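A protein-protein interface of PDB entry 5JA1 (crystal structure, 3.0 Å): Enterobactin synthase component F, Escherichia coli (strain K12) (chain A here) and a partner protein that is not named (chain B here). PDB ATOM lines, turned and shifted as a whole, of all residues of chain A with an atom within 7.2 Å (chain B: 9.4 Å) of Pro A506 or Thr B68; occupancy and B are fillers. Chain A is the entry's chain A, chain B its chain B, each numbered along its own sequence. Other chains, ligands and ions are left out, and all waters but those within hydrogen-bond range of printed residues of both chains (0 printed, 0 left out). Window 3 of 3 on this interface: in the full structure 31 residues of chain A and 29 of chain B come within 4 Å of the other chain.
The backbone carbonyl oxygen (O) of Pro A506 lies within hydrogen-bond range of the side-chain hydroxyl (OG1) of Thr B68, at 3.1 Å. The backbone carbonyl oxygen (O) of Gly A507 lies close to the backbone carbonyl oxygen (O) of Pro B64 (3.4 Å). O of Thr B68 lies within hydrogen-bond range of NE2 of His A598 (3.4 Å). The backbone carbonyl oxygen of Gly A507 sits close to the backbone NH of Thr B65 (3.3 Å). ND1 of His A597 lies within hydrogen-bond range of O of Phe B67 (3.1 Å). O of Gln B69 lies close to NE2 of His A597 (3.3 Å).
N of Gly A507 lies within hydrogen-bond range of O of Gly A531 (2.8 Å). A ring nitrogen (ND1) of His A598 lies within hydrogen-bond range of the backbone NH (N) of Gln A595, 3.3 Å away. O of His A597 lies within hydrogen-bond range of NE2 of Gln A813 (3.3 Å). The side-chain amide oxygen (OE1) of Gln A813 is in hydrogen-bond range of the side-chain hydroxyl (OG1) of Thr A599.
Among the printed residues, merely in contact across the chains: Gly A507 with Thr B68 (3.99 Å), Ser A509 with Pro B64 (3.5 Å), His A597 with Thr B68 (3.4 Å), His A597 with Leu B70 (3.6 Å), His A598 with Phe B67 (3.7 Å), Thr A599 with Pro B64 (3.5 Å), Thr A599 with Phe B67 (3.9 Å) and Gln A813 with Phe B67 (3.7 Å).
Of chain B, only Thr B68 (3.1 Å) comes within 4 Å of Pro A506. No residue of chain B comes within 4 Å of Gly A531. Of the printed residues of chain A, Thr B65 touches Gly A507 (3.2 Å). Of the printed residues of chain A, Thr B68 touches Pro A506, Gly A507, His A597 and His A598. Printed residues of chain A within 4 Å of Gln B69: His A597 (3.2 Å). Printed residues of chain A within 4 Å of Leu B70: His A597.
Hydrophobic or aromatic side chains of chain B within 4 Å of the printed part of chain A: Pro B64 and Phe B67. Of the 20 printed residues of chain A, 7 touch a printed residue of chain B. Hydrophobic or aromatic side chains of chain A within 4 Å of the printed part of chain B: His A597 and His A598.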
ATOM      1  N   ARG A 500      35.196 -22.067   8.847  1.00  0.00           N
ATOM      2  CA  ARG A 500      33.887 -22.643   8.565  1.00  0.00           C
ATOM      3  C   ARG A 500      33.468 -23.611   9.665  1.00  0.00           C
ATOM      4  O   ARG A 500      32.298 -23.641  10.064  1.00  0.00           O
ATOM      5  CB  ARG A 500      33.907 -23.348   7.207  1.00  0.00           C
ATOM      6  CG  ARG A 500      32.609 -24.053   6.845  1.00  0.00           C
ATOM      7  CD  ARG A 500      32.821 -25.042   5.708  1.00  0.00           C
ATOM      8  NE  ARG A 500      33.088 -24.388   4.429  1.00  0.00           N
ATOM      9  CZ  ARG A 500      33.515 -25.024   3.343  1.00  0.00           C
ATOM     10  NH1 ARG A 500      33.735 -26.331   3.383  1.00  0.00           N
ATOM     11  NH2 ARG A 500      33.729 -24.357   2.218  1.00  0.00           N
ATOM     12  N   GLY A 503      31.816 -21.795  12.433  1.00  0.00           N
ATOM     13  CA  GLY A 503      30.587 -21.072  12.187  1.00  0.00           C
ATOM     14  C   GLY A 503      30.713 -19.795  11.392  1.00  0.00           C
ATOM     15  O   GLY A 503      29.871 -18.901  11.538  1.00  0.00           O
ATOM     16  N   VAL A 504      31.734 -19.672  10.551  1.00  0.00           N
ATOM     17  CA  VAL A 504      31.887 -18.513   9.681  1.00  0.00           C
ATOM     18  C   VAL A 504      31.246 -18.848   8.339  1.00  0.00           C
ATOM     19  O   VAL A 504      31.813 -19.592   7.537  1.00  0.00           O
ATOM     20  CB  VAL A 504      33.357 -18.116   9.513  1.00  0.00           C
ATOM     21  CG1 VAL A 504      33.485 -17.000   8.489  1.00  0.00           C
ATOM     22  CG2 VAL A 504      33.942 -17.683  10.847  1.00  0.00           C
ATOM     23  N   LYS A 505      30.059 -18.308   8.100  1.00  0.00           N
ATOM     24  CA  LYS A 505      29.366 -18.492   6.838  1.00  0.00           C
ATOM     25  C   LYS A 505      29.610 -17.303   5.921  1.00  0.00           C
ATOM     26  O   LYS A 505      30.012 -16.227   6.376  1.00  0.00           O
ATOM     27  CB  LYS A 505      27.862 -18.677   7.075  1.00  0.00           C
ATOM     28  CG  LYS A 505      27.207 -17.583   7.899  1.00  0.00           C
ATOM     29  CD  LYS A 505      25.715 -17.840   8.063  1.00  0.00           C
ATOM     30  CE  LYS A 505      25.060 -16.802   8.963  1.00  0.00           C
ATOM     31  NZ  LYS A 505      25.604 -16.842  10.349  1.00  0.00           N
ATOM     32  N   PRO A 506      29.412 -17.471   4.613  1.00  0.00           N
ATOM     33  CA  PRO A 506      29.579 -16.342   3.689  1.00  0.00           C
ATOM     34  C   PRO A 506      28.687 -15.168   4.067  1.00  0.00           C
ATOM     35  O   PRO A 506      27.477 -15.318   4.251  1.00  0.00           O
ATOM     36  CB  PRO A 506      29.185 -16.938   2.333  1.00  0.00           C
ATOM     37  CG  PRO A 506      29.530 -18.374   2.456  1.00  0.00           C
ATOM     38  CD  PRO A 506      29.235 -18.744   3.890  1.00  0.00           C
ATOM     39  N   GLY A 507      29.300 -13.990   4.181  1.00  0.00           N
ATOM     40  CA  GLY A 507      28.604 -12.781   4.576  1.00  0.00           C
ATOM     41  C   GLY A 507      28.872 -12.333   5.996  1.00  0.00           C
ATOM     42  O   GLY A 507      28.308 -11.317   6.421  1.00  0.00           O
ATOM     43  N   ASP A 508      29.708 -13.042   6.742  1.00  0.00           N
ATOM     44  CA  ASP A 508      29.985 -12.682   8.122  1.00  0.00           C
ATOM     45  C   ASP A 508      31.217 -11.784   8.219  1.00  0.00           C
ATOM     46  O   ASP A 508      31.952 -11.574   7.253  1.00  0.00           O
ATOM     47  CB  ASP A 508      30.182 -13.934   8.976  1.00  0.00           C
ATOM     48  CG  ASP A 508      28.887 -14.666   9.241  1.00  0.00           C
ATOM     49  OD1 ASP A 508      27.814 -14.099   8.942  1.00  0.00           O
ATOM     50  OD2 ASP A 508      28.943 -15.800   9.761  1.00  0.00           O
ATOM     51  N   SER A 509      31.432 -11.246   9.416  1.00  0.00           N
ATOM     52  CA  SER A 509      32.619 -10.471   9.731  1.00  0.00           C
ATOM     53  C   SER A 509      33.514 -11.275  10.663  1.00  0.00           C
ATOM     54  O   SER A 509      33.033 -12.040  11.502  1.00  0.00           O
ATOM     55  CB  SER A 509      32.257  -9.136  10.385  1.00  0.00           C
ATOM     56  OG  SER A 509      31.388  -8.383   9.559  1.00  0.00           O
ATOM     57  N   GLU A 529      38.634 -16.193   1.661  1.00  0.00           N
ATOM     58  CA  GLU A 529      38.390 -17.516   1.096  1.00  0.00           C
ATOM     59  C   GLU A 529      37.081 -18.110   1.601  1.00  0.00           C
ATOM     60  O   GLU A 529      36.397 -18.825   0.858  1.00  0.00           O
ATOM     61  CB  GLU A 529      39.556 -18.448   1.429  1.00  0.00           C
ATOM     62  CG  GLU A 529      39.552 -19.743   0.644  1.00  0.00           C
ATOM     63  CD  GLU A 529      39.967 -19.545  -0.799  1.00  0.00           C
ATOM     64  OE1 GLU A 529      40.661 -18.547  -1.088  1.00  0.00           O
ATOM     65  OE2 GLU A 529      39.598 -20.388  -1.643  1.00  0.00           O
ATOM     66  N   ALA A 530      36.712 -17.819   2.848  1.00  0.00           N
ATOM     67  CA  ALA A 530      35.459 -18.293   3.418  1.00  0.00           C
ATOM     68  C   ALA A 530      34.264 -17.427   3.041  1.00  0.00           C
ATOM     69  O   ALA A 530      33.147 -17.719   3.482  1.00  0.00           O
ATOM     70  CB  ALA A 530      35.574 -18.375   4.943  1.00  0.00           C
ATOM     71  N   GLY A 531      34.460 -16.384   2.240  1.00  0.00           N
ATOM     72  CA  GLY A 531      33.359 -15.517   1.872  1.00  0.00           C
ATOM     73  C   GLY A 531      32.960 -14.528   2.941  1.00  0.00           C
ATOM     74  O   GLY A 531      31.814 -14.066   2.954  1.00  0.00           O
ATOM     75  N   ALA A 532      33.874 -14.189   3.841  1.00  0.00           N
ATOM     76  CA  ALA A 532      33.620 -13.249   4.919  1.00  0.00           C
ATOM     77  C   ALA A 532      34.472 -11.997   4.740  1.00  0.00           C
ATOM     78  O   ALA A 532      35.428 -11.967   3.962  1.00  0.00           O
ATOM     79  CB  ALA A 532      33.900 -13.896   6.280  1.00  0.00           C
ATOM     80  N   ALA A 533      34.106 -10.954   5.474  1.00  0.00           N
ATOM     81  CA  ALA A 533      34.853  -9.705   5.493  1.00  0.00           C
ATOM     82  C   ALA A 533      35.645  -9.608   6.788  1.00  0.00           C
ATOM     83  O   ALA A 533      35.165 -10.017   7.850  1.00  0.00           O
ATOM     84  CB  ALA A 533      33.913  -8.507   5.359  1.00  0.00           C
ATOM     85  N   LEU A 593      33.739 -19.868  -2.214  1.00  0.00           N
ATOM     86  CA  LEU A 593      32.678 -19.281  -1.406  1.00  0.00           C
ATOM     87  C   LEU A 593      32.534 -17.782  -1.619  1.00  0.00           C
ATOM     88  O   LEU A 593      31.496 -17.215  -1.257  1.00  0.00           O
ATOM     89  CB  LEU A 593      32.930 -19.551   0.079  1.00  0.00           C
ATOM     90  CG  LEU A 593      32.861 -21.008   0.532  1.00  0.00           C
ATOM     91  CD1 LEU A 593      33.189 -21.114   2.012  1.00  0.00           C
ATOM     92  CD2 LEU A 593      31.488 -21.591   0.239  1.00  0.00           C
ATOM     93  N   SER A 594      33.543 -17.135  -2.197  1.00  0.00           N
ATOM     94  CA  SER A 594      33.532 -15.689  -2.352  1.00  0.00           C
ATOM     95  C   SER A 594      32.710 -15.285  -3.569  1.00  0.00           C
ATOM     96  O   SER A 594      32.757 -15.937  -4.615  1.00  0.00           O
ATOM     97  CB  SER A 594      34.960 -15.159  -2.482  1.00  0.00           C
ATOM     98  OG  SER A 594      34.991 -13.743  -2.448  1.00  0.00           O
ATOM     99  N   GLN A 595      31.954 -14.201  -3.424  1.00  0.00           N
ATOM    100  CA  GLN A 595      31.132 -13.648  -4.486  1.00  0.00           C
ATOM    101  C   GLN A 595      31.433 -12.165  -4.646  1.00  0.00           C
ATOM    102  O   GLN A 595      31.854 -11.509  -3.687  1.00  0.00           O
ATOM    103  CB  GLN A 595      29.637 -13.849  -4.197  1.00  0.00           C
ATOM    104  CG  GLN A 595      29.177 -15.296  -4.303  1.00  0.00           C
ATOM    105  CD  GLN A 595      29.396 -15.877  -5.688  1.00  0.00           C
ATOM    106  OE1 GLN A 595      29.329 -15.169  -6.692  1.00  0.00           O
ATOM    107  NE2 GLN A 595      29.666 -17.177  -5.746  1.00  0.00           N
ATOM    108  N   HIS A 597      29.516  -9.570  -4.924  1.00  0.00           N
ATOM    109  CA  HIS A 597      28.652  -8.678  -4.158  1.00  0.00           C
ATOM    110  C   HIS A 597      28.945  -8.695  -2.664  1.00  0.00           C
ATOM    111  O   HIS A 597      28.375  -7.880  -1.931  1.00  0.00           O
ATOM    112  CB  HIS A 597      27.184  -9.044  -4.394  1.00  0.00           C
ATOM    113  CG  HIS A 597      26.918 -10.515  -4.343  1.00  0.00           C
ATOM    114  ND1 HIS A 597      26.730 -11.200  -3.160  1.00  0.00           N
ATOM    115  CD2 HIS A 597      26.824 -11.438  -5.330  1.00  0.00           C
ATOM    116  CE1 HIS A 597      26.523 -12.478  -3.422  1.00  0.00           C
ATOM    117  NE2 HIS A 597      26.575 -12.649  -4.732  1.00  0.00           N
ATOM    118  N   HIS A 598      29.813  -9.589  -2.201  1.00  0.00           N
ATOM    119  CA  HIS A 598      30.123  -9.677  -0.784  1.00  0.00           C
ATOM    120  C   HIS A 598      30.918  -8.459  -0.320  1.00  0.00           C
ATOM    121  O   HIS A 598      31.581  -7.774  -1.105  1.00  0.00           O
ATOM    122  CB  HIS A 598      30.918 -10.948  -0.484  1.00  0.00           C
ATOM    123  CG  HIS A 598      30.101 -12.201  -0.536  1.00  0.00           C
ATOM    124  ND1 HIS A 598      30.667 -13.458  -0.510  1.00  0.00           N
ATOM    125  CD2 HIS A 598      28.763 -12.393  -0.604  1.00  0.00           C
ATOM    126  CE1 HIS A 598      29.713 -14.369  -0.564  1.00  0.00           C
ATOM    127  NE2 HIS A 598      28.548 -13.750  -0.621  1.00  0.00           N
ATOM    128  N   THR A 599      30.843  -8.194   0.980  1.00  0.00           N
ATOM    129  CA  THR A 599      31.696  -7.192   1.598  1.00  0.00           C
ATOM    130  C   THR A 599      33.101  -7.757   1.747  1.00  0.00           C
ATOM    131  O   THR A 599      33.276  -8.896   2.191  1.00  0.00           O
ATOM    132  CB  THR A 599      31.141  -6.776   2.961  1.00  0.00           C
ATOM    133  OG1 THR A 599      29.794  -6.311   2.811  1.00  0.00           O
ATOM    134  CG2 THR A 599      31.987  -5.668   3.567  1.00  0.00           C
ATOM    135  N   GLN A 813      30.129   0.270   0.039  1.00  0.00           N
ATOM    136  CA  GLN A 813      28.728  -0.104   0.176  1.00  0.00           C
ATOM    137  C   GLN A 813      27.987   0.854   1.102  1.00  0.00           C
ATOM    138  O   GLN A 813      26.764   0.994   0.995  1.00  0.00           O
ATOM    139  CB  GLN A 813      28.614  -1.544   0.682  1.00  0.00           C
ATOM    140  CG  GLN A 813      29.072  -2.589  -0.324  1.00  0.00           C
ATOM    141  CD  GLN A 813      29.323  -3.943   0.313  1.00  0.00           C
ATOM    142  OE1 GLN A 813      29.590  -4.036   1.511  1.00  0.00           O
ATOM    143  NE2 GLN A 813      29.238  -5.003  -0.486  1.00  0.00           N
ATOM    144  N   THR B  61      19.043  -2.568   6.268  1.00  0.00           N
ATOM    145  CA  THR B  61      19.696  -3.609   5.482  1.00  0.00           C
ATOM    146  C   THR B  61      21.149  -3.275   5.167  1.00  0.00           C
ATOM    147  O   THR B  61      21.689  -3.751   4.160  1.00  0.00           O
ATOM    148  CB  THR B  61      18.921  -3.854   4.186  1.00  0.00           C
ATOM    149  OG1 THR B  61      18.913  -2.658   3.398  1.00  0.00           O
ATOM    150  CG2 THR B  61      17.487  -4.260   4.487  1.00  0.00           C
ATOM    151  N   THR B  63      24.135  -3.955   6.592  1.00  0.00           N
ATOM    152  CA  THR B  63      25.156  -4.764   7.238  1.00  0.00           C
ATOM    153  C   THR B  63      25.804  -5.711   6.231  1.00  0.00           C
ATOM    154  O   THR B  63      25.208  -6.031   5.196  1.00  0.00           O
ATOM    155  CB  THR B  63      24.556  -5.573   8.399  1.00  0.00           C
ATOM    156  OG1 THR B  63      23.567  -6.479   7.894  1.00  0.00           O
ATOM    157  CG2 THR B  63      23.917  -4.644   9.424  1.00  0.00           C
ATOM    158  N   PRO B  64      27.030  -6.178   6.495  1.00  0.00           N
ATOM    159  CA  PRO B  64      27.695  -7.059   5.520  1.00  0.00           C
ATOM    160  C   PRO B  64      26.983  -8.383   5.310  1.00  0.00           C
ATOM    161  O   PRO B  64      27.164  -9.000   4.252  1.00  0.00           O
ATOM    162  CB  PRO B  64      29.093  -7.259   6.124  1.00  0.00           C
ATOM    163  CG  PRO B  64      28.912  -7.013   7.575  1.00  0.00           C
ATOM    164  CD  PRO B  64      27.887  -5.924   7.666  1.00  0.00           C
ATOM    165  N   THR B  65      26.181  -8.841   6.270  1.00  0.00           N
ATOM    166  CA  THR B  65      25.392 -10.052   6.077  1.00  0.00           C
ATOM    167  C   THR B  65      24.151  -9.813   5.228  1.00  0.00           C
ATOM    168  O   THR B  65      23.446 -10.775   4.908  1.00  0.00           O
ATOM    169  CB  THR B  65      24.981 -10.651   7.428  1.00  0.00           C
ATOM    170  OG1 THR B  65      24.419 -11.954   7.223  1.00  0.00           O
ATOM    171  CG2 THR B  65      23.953  -9.764   8.114  1.00  0.00           C
ATOM    172  N   ASN B  66      23.867  -8.562   4.862  1.00  0.00           N
ATOM    173  CA  ASN B  66      22.775  -8.258   3.947  1.00  0.00           C
ATOM    174  C   ASN B  66      23.217  -8.224   2.492  1.00  0.00           C
ATOM    175  O   ASN B  66      22.382  -8.407   1.600  1.00  0.00           O
ATOM    176  CB  ASN B  66      22.128  -6.917   4.314  1.00  0.00           C
ATOM    177  CG  ASN B  66      21.299  -6.997   5.580  1.00  0.00           C
ATOM    178  OD1 ASN B  66      21.628  -6.377   6.591  1.00  0.00           O
ATOM    179  ND2 ASN B  66      20.216  -7.765   5.532  1.00  0.00           N
ATOM    180  N   PHE B  67      24.503  -7.996   2.233  1.00  0.00           N
ATOM    181  CA  PHE B  67      25.058  -8.071   0.889  1.00  0.00           C
ATOM    182  C   PHE B  67      25.468  -9.488   0.510  1.00  0.00           C
ATOM    183  O   PHE B  67      26.191  -9.673  -0.473  1.00  0.00           O
ATOM    184  CB  PHE B  67      26.259  -7.131   0.758  1.00  0.00           C
ATOM    185  CG  PHE B  67      25.923  -5.684   0.979  1.00  0.00           C
ATOM    186  CD1 PHE B  67      25.421  -4.911  -0.054  1.00  0.00           C
ATOM    187  CD2 PHE B  67      26.110  -5.099   2.220  1.00  0.00           C
ATOM    188  CE1 PHE B  67      25.109  -3.583   0.144  1.00  0.00           C
ATOM    189  CE2 PHE B  67      25.801  -3.770   2.427  1.00  0.00           C
ATOM    190  CZ  PHE B  67      25.300  -3.011   1.387  1.00  0.00           C
ATOM    191  N   THR B  68      25.014 -10.490   1.264  1.00  0.00           N
ATOM    192  CA  THR B  68      25.436 -11.867   1.043  1.00  0.00           C
ATOM    193  C   THR B  68      24.778 -12.513  -0.168  1.00  0.00           C
ATOM    194  O   THR B  68      25.194 -13.610  -0.556  1.00  0.00           O
ATOM    195  CB  THR B  68      25.136 -12.715   2.284  1.00  0.00           C
ATOM    196  OG1 THR B  68      25.710 -14.018   2.124  1.00  0.00           O
ATOM    197  CG2 THR B  68      23.636 -12.861   2.474  1.00  0.00           C
ATOM    198  N   GLN B  69      23.775 -11.879  -0.777  1.00  0.00           N
ATOM    199  CA  GLN B  69      23.001 -12.590  -1.789  1.00  0.00           C
ATOM    200  C   GLN B  69      22.885 -11.855  -3.119  1.00  0.00           C
ATOM    201  O   GLN B  69      23.387 -12.340  -4.139  1.00  0.00           O
ATOM    202  CB  GLN B  69      21.605 -12.906  -1.252  1.00  0.00           C
ATOM    203  CG  GLN B  69      20.939 -14.034  -2.006  1.00  0.00           C
ATOM    204  CD  GLN B  69      21.875 -15.214  -2.201  1.00  0.00           C
ATOM    205  OE1 GLN B  69      22.478 -15.377  -3.264  1.00  0.00           O
ATOM    206  NE2 GLN B  69      22.007 -16.041  -1.170  1.00  0.00           N
ATOM    207  N   LEU B  70      22.212 -10.707  -3.135  1.00  0.00           N
ATOM    208  CA  LEU B  70      21.903 -10.030  -4.395  1.00  0.00           C
ATOM    209  C   LEU B  70      23.170  -9.577  -5.113  1.00  0.00           C
ATOM    210  O   LEU B  70      23.526 -10.123  -6.159  1.00  0.00           O
ATOM    211  CB  LEU B  70      20.974  -8.834  -4.155  1.00  0.00           C
ATOM    212  CG  LEU B  70      20.369  -8.182  -5.406  1.00  0.00           C
ATOM    213  CD1 LEU B  70      18.920  -7.785  -5.161  1.00  0.00           C
ATOM    214  CD2 LEU B  70      21.179  -6.971  -5.858  1.00  0.00           C
